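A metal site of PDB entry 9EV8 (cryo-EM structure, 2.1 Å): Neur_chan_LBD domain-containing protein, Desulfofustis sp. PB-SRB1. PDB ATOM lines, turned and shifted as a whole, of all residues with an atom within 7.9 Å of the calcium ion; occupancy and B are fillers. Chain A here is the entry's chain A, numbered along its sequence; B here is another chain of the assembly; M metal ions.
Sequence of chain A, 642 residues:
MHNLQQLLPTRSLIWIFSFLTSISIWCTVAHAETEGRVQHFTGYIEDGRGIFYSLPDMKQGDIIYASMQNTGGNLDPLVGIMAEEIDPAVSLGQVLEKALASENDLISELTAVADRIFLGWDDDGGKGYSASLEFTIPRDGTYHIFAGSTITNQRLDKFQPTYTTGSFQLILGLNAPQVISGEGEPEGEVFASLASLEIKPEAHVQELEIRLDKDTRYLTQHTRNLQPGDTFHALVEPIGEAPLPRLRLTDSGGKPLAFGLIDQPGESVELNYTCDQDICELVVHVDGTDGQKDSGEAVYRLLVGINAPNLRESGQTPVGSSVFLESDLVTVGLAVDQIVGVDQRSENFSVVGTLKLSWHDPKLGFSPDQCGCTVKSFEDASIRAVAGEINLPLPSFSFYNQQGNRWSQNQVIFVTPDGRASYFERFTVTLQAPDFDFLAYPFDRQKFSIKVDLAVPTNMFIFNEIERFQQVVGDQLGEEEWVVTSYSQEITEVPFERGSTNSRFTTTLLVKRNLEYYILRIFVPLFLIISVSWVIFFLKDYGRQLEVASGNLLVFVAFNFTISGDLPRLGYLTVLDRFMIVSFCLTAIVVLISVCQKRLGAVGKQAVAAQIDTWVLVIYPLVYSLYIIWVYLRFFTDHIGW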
ATOM      1  N   MET A  68     -15.958 -26.826 -13.866  1.00  0.00           N
ATOM      2  CA  MET A  68     -16.433 -27.743 -12.834  1.00  0.00           C
ATOM      3  C   MET A  68     -16.547 -29.144 -13.425  1.00  0.00           C
ATOM      4  O   MET A  68     -17.224 -29.343 -14.430  1.00  0.00           O
ATOM      5  CB  MET A  68     -17.794 -27.271 -12.289  1.00  0.00           C
ATOM      6  CG  MET A  68     -18.288 -28.014 -11.066  1.00  0.00           C
ATOM      7  SD  MET A  68     -19.782 -27.248 -10.406  1.00  0.00           S
ATOM      8  CE  MET A  68     -20.277 -28.437  -9.171  1.00  0.00           C
ATOM      9  N   LEU A  75     -23.242 -36.685 -10.415  1.00  0.00           N
ATOM     10  CA  LEU A  75     -23.431 -35.237 -10.427  1.00  0.00           C
ATOM     11  C   LEU A  75     -23.325 -34.658 -11.840  1.00  0.00           C
ATOM     12  O   LEU A  75     -22.456 -35.059 -12.616  1.00  0.00           O
ATOM     13  CB  LEU A  75     -22.403 -34.584  -9.514  1.00  0.00           C
ATOM     14  CG  LEU A  75     -22.387 -33.056  -9.466  1.00  0.00           C
ATOM     15  CD1 LEU A  75     -23.720 -32.528  -8.980  1.00  0.00           C
ATOM     16  CD2 LEU A  75     -21.263 -32.570  -8.585  1.00  0.00           C
ATOM     17  N   ASP A  76     -24.216 -33.730 -12.155  1.00  0.00           N
ATOM     18  CA  ASP A  76     -24.173 -32.986 -13.403  1.00  0.00           C
ATOM     19  C   ASP A  76     -23.889 -31.511 -13.105  1.00  0.00           C
ATOM     20  O   ASP A  76     -24.791 -30.796 -12.655  1.00  0.00           O
ATOM     21  CB  ASP A  76     -25.488 -33.129 -14.160  1.00  0.00           C
ATOM     22  CG  ASP A  76     -25.339 -32.946 -15.653  1.00  0.00           C
ATOM     23  OD1 ASP A  76     -24.416 -32.209 -16.076  1.00  0.00           O
ATOM     24  OD2 ASP A  76     -26.129 -33.542 -16.414  1.00  0.00           O
ATOM     25  N   PRO A  77     -22.669 -31.032 -13.329  1.00  0.00           N
ATOM     26  CA  PRO A  77     -22.291 -29.692 -12.858  1.00  0.00           C
ATOM     27  C   PRO A  77     -23.088 -28.571 -13.513  1.00  0.00           C
ATOM     28  O   PRO A  77     -23.515 -28.652 -14.658  1.00  0.00           O
ATOM     29  CB  PRO A  77     -20.812 -29.591 -13.216  1.00  0.00           C
ATOM     30  CG  PRO A  77     -20.356 -31.008 -13.316  1.00  0.00           C
ATOM     31  CD  PRO A  77     -21.517 -31.765 -13.870  1.00  0.00           C
ATOM     32  N   LEU A  78     -23.285 -27.492 -12.740  1.00  0.00           N
ATOM     33  CA  LEU A  78     -23.834 -26.234 -13.206  1.00  0.00           C
ATOM     34  C   LEU A  78     -23.181 -25.092 -12.453  1.00  0.00           C
ATOM     35  O   LEU A  78     -22.951 -25.199 -11.236  1.00  0.00           O
ATOM     36  CB  LEU A  78     -25.363 -26.183 -13.006  1.00  0.00           C
ATOM     37  CG  LEU A  78     -26.052 -24.846 -13.275  1.00  0.00           C
ATOM     38  CD1 LEU A  78     -25.866 -24.420 -14.720  1.00  0.00           C
ATOM     39  CD2 LEU A  78     -27.530 -24.924 -12.924  1.00  0.00           C
ATOM     40  N   VAL A  79     -22.859 -24.003 -13.156  1.00  0.00           N
ATOM     41  CA  VAL A  79     -22.184 -22.860 -12.565  1.00  0.00           C
ATOM     42  C   VAL A  79     -22.877 -21.580 -12.996  1.00  0.00           C
ATOM     43  O   VAL A  79     -23.307 -21.450 -14.148  1.00  0.00           O
ATOM     44  CB  VAL A  79     -20.688 -22.841 -12.940  1.00  0.00           C
ATOM     45  CG1 VAL A  79     -20.500 -22.776 -14.459  1.00  0.00           C
ATOM     46  CG2 VAL A  79     -19.966 -21.690 -12.256  1.00  0.00           C
ATOM     47  N   ASP A 122     -23.361 -21.609 -17.452  1.00  0.00           N
ATOM     48  CA  ASP A 122     -23.026 -22.614 -18.455  1.00  0.00           C
ATOM     49  C   ASP A 122     -23.373 -23.988 -17.898  1.00  0.00           C
ATOM     50  O   ASP A 122     -23.139 -24.254 -16.721  1.00  0.00           O
ATOM     51  CB  ASP A 122     -21.549 -22.556 -18.845  1.00  0.00           C
ATOM     52  CG  ASP A 122     -21.197 -23.586 -19.898  1.00  0.00           C
ATOM     53  OD1 ASP A 122     -21.661 -23.440 -21.051  1.00  0.00           O
ATOM     54  OD2 ASP A 122     -20.445 -24.532 -19.594  1.00  0.00           O
ATOM     55  N   ASP A 123     -23.910 -24.854 -18.753  1.00  0.00           N
ATOM     56  CA  ASP A 123     -24.317 -26.199 -18.354  1.00  0.00           C
ATOM     57  C   ASP A 123     -23.319 -27.250 -18.829  1.00  0.00           C
ATOM     58  O   ASP A 123     -22.758 -27.967 -18.000  1.00  0.00           O
ATOM     59  CB  ASP A 123     -25.721 -26.496 -18.879  1.00  0.00           C
ATOM     60  CG  ASP A 123     -26.399 -27.621 -18.134  1.00  0.00           C
ATOM     61  OD1 ASP A 123     -25.691 -28.475 -17.566  1.00  0.00           O
ATOM     62  OD2 ASP A 123     -27.638 -27.652 -18.119  1.00  0.00           O
ATOM     63  N   ASP A 124     -23.080 -27.366 -20.128  1.00  0.00           N
ATOM     64  CA  ASP A 124     -22.340 -28.487 -20.703  1.00  0.00           C
ATOM     65  C   ASP A 124     -21.266 -28.017 -21.673  1.00  0.00           C
ATOM     66  O   ASP A 124     -20.997 -28.654 -22.694  1.00  0.00           O
ATOM     67  CB  ASP A 124     -23.296 -29.434 -21.412  1.00  0.00           C
ATOM     68  CG  ASP A 124     -24.317 -30.035 -20.477  1.00  0.00           C
ATOM     69  OD1 ASP A 124     -23.964 -30.352 -19.328  1.00  0.00           O
ATOM     70  OD2 ASP A 124     -25.493 -30.180 -20.880  1.00  0.00           O
ATOM     71  N   GLY A 125     -20.602 -26.896 -21.360  1.00  0.00           N
ATOM     72  CA  GLY A 125     -19.630 -26.343 -22.278  1.00  0.00           C
ATOM     73  C   GLY A 125     -18.298 -27.058 -22.333  1.00  0.00           C
ATOM     74  O   GLY A 125     -17.493 -26.752 -23.210  1.00  0.00           O
ATOM     75  N   GLY A 126     -18.052 -28.009 -21.426  1.00  0.00           N
ATOM     76  CA  GLY A 126     -16.789 -28.689 -21.343  1.00  0.00           C
ATOM     77  C   GLY A 126     -16.854 -30.106 -21.872  1.00  0.00           C
ATOM     78  O   GLY A 126     -17.773 -30.496 -22.608  1.00  0.00           O
ATOM     79  N   GLY A 128     -17.825 -33.600 -21.953  1.00  0.00           N
ATOM     80  CA  GLY A 128     -18.933 -34.307 -21.368  1.00  0.00           C
ATOM     81  C   GLY A 128     -19.977 -33.350 -20.831  1.00  0.00           C
ATOM     82  O   GLY A 128     -20.391 -32.424 -21.528  1.00  0.00           O
ATOM     83  N   TYR A 129     -20.407 -33.561 -19.588  1.00  0.00           N
ATOM     84  CA  TYR A 129     -21.406 -32.723 -18.942  1.00  0.00           C
ATOM     85  C   TYR A 129     -20.787 -31.634 -18.079  1.00  0.00           C
ATOM     86  O   TYR A 129     -21.501 -30.950 -17.343  1.00  0.00           O
ATOM     87  CB  TYR A 129     -22.355 -33.591 -18.108  1.00  0.00           C
ATOM     88  CG  TYR A 129     -23.164 -34.575 -18.915  1.00  0.00           C
ATOM     89  CD1 TYR A 129     -23.454 -34.337 -20.254  1.00  0.00           C
ATOM     90  CD2 TYR A 129     -23.650 -35.739 -18.350  1.00  0.00           C
ATOM     91  CE1 TYR A 129     -24.193 -35.235 -20.997  1.00  0.00           C
ATOM     92  CE2 TYR A 129     -24.397 -36.641 -19.078  1.00  0.00           C
ATOM     93  CZ  TYR A 129     -24.659 -36.384 -20.405  1.00  0.00           C
ATOM     94  OH  TYR A 129     -25.400 -37.277 -21.134  1.00  0.00           O
ATOM     95  N   SER A 130     -19.469 -31.458 -18.160  1.00  0.00           N
ATOM     96  CA  SER A 130     -18.775 -30.457 -17.358  1.00  0.00           C
ATOM     97  C   SER A 130     -19.027 -29.058 -17.915  1.00  0.00           C
ATOM     98  O   SER A 130     -19.222 -28.882 -19.111  1.00  0.00           O
ATOM     99  CB  SER A 130     -17.282 -30.745 -17.318  1.00  0.00           C
ATOM    100  OG  SER A 130     -16.728 -30.731 -18.627  1.00  0.00           O
ATOM    101  N   ALA A 131     -19.017 -28.074 -17.019  1.00  0.00           N
ATOM    102  CA  ALA A 131     -19.291 -26.692 -17.371  1.00  0.00           C
ATOM    103  C   ALA A 131     -18.010 -25.871 -17.478  1.00  0.00           C
ATOM    104  O   ALA A 131     -16.999 -26.170 -16.837  1.00  0.00           O
ATOM    105  CB  ALA A 131     -20.226 -26.052 -16.343  1.00  0.00           C
ATOM    106  N   GLY A 148     -23.513 -26.033  -8.264  1.00  0.00           N
ATOM    107  CA  GLY A 148     -24.599 -26.909  -7.892  1.00  0.00           C
ATOM    108  C   GLY A 148     -24.923 -27.907  -8.971  1.00  0.00           C
ATOM    109  O   GLY A 148     -24.073 -28.250  -9.804  1.00  0.00           O
ATOM    110  N   SER A 149     -26.168 -28.381  -8.952  1.00  0.00           N
ATOM    111  CA  SER A 149     -26.635 -29.420  -9.849  1.00  0.00           C
ATOM    112  C   SER A 149     -27.755 -28.881 -10.734  1.00  0.00           C
ATOM    113  O   SER A 149     -28.642 -28.163 -10.268  1.00  0.00           O
ATOM    114  CB  SER A 149     -27.136 -30.629  -9.056  1.00  0.00           C
ATOM    115  OG  SER A 149     -27.723 -31.597  -9.907  1.00  0.00           O
ATOM    116  N   THR A 150     -27.714 -29.239 -12.020  1.00  0.00           N
ATOM    117  CA  THR A 150     -28.792 -28.912 -12.931  1.00  0.00           C
ATOM    118  C   THR A 150     -29.909 -29.954 -12.847  1.00  0.00           C
ATOM    119  O   THR A 150     -29.830 -30.932 -12.100  1.00  0.00           O
ATOM    120  CB  THR A 150     -28.277 -28.811 -14.361  1.00  0.00           C
ATOM    121  OG1 THR A 150     -29.373 -28.612 -15.258  1.00  0.00           O
ATOM    122  CG2 THR A 150     -27.538 -30.077 -14.750  1.00  0.00           C
ATOM    123  N   ILE A 151     -30.969 -29.733 -13.619  1.00  0.00           N
ATOM    124  CA  ILE A 151     -32.095 -30.643 -13.697  1.00  0.00           C
ATOM    125  C   ILE A 151     -31.971 -31.451 -14.981  1.00  0.00           C
ATOM    126  O   ILE A 151     -31.973 -30.888 -16.074  1.00  0.00           O
ATOM    127  CB  ILE A 151     -33.437 -29.883 -13.650  1.00  0.00           C
ATOM    128  CG1 ILE A 151     -33.540 -29.087 -12.344  1.00  0.00           C
ATOM    129  CG2 ILE A 151     -34.596 -30.844 -13.790  1.00  0.00           C
ATOM    130  CD1 ILE A 151     -34.811 -28.268 -12.240  1.00  0.00           C
ATOM    131  N   THR A 152     -31.887 -32.774 -14.849  1.00  0.00           N
ATOM    132  CA  THR A 152     -31.628 -33.638 -15.988  1.00  0.00           C
ATOM    133  C   THR A 152     -32.444 -34.923 -15.866  1.00  0.00           C
ATOM    134  O   THR A 152     -32.994 -35.230 -14.801  1.00  0.00           O
ATOM    135  CB  THR A 152     -30.145 -34.005 -16.110  1.00  0.00           C
ATOM    136  OG1 THR A 152     -29.683 -34.581 -14.883  1.00  0.00           O
ATOM    137  CG2 THR A 152     -29.303 -32.782 -16.433  1.00  0.00           C
ATOM    138  N   LYS B 255     -30.157 -37.266 -20.822  1.00  0.00           N
ATOM    139  CA  LYS B 255     -30.145 -35.806 -20.672  1.00  0.00           C
ATOM    140  C   LYS B 255     -30.963 -35.186 -21.792  1.00  0.00           C
ATOM    141  O   LYS B 255     -30.638 -35.375 -22.969  1.00  0.00           O
ATOM    142  CB  LYS B 255     -28.716 -35.253 -20.655  1.00  0.00           C
HETATM  143 CA    CA M   1     -24.390 -29.905 -17.193  1.00  0.00          CA
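Thr 150 touches the calcium ion.
Along chain A the residues within 4 Å of the calcium ion span positions 76 to 150.
The nearest printed residue that does not touch the calcium ion is Leu 78 (5.2 Å).
The calcium ion is bound by OD1 of Asp 123 (2.0 Å), OD1 of Asp 124 (2.2 Å), OD1 of Asp 76 (2.6 Å) and O of Asp 123 (2.7 Å).
Slightly farther from the calcium ion lies the backbone carbonyl oxygen (O) of Pro 77 (3.0 Å).
Slightly farther from the calcium ion lies O of Tyr 129 (3.1 Å).
O of Asp 76 lies within hydrogen-bond range of N of Thr 150, at 3.4 Å.
The side-chain carboxylate (OD2) of Asp 123 lies within hydrogen-bond range of the side-chain hydroxyl (OG1) of Thr 150 (3.5 Å).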
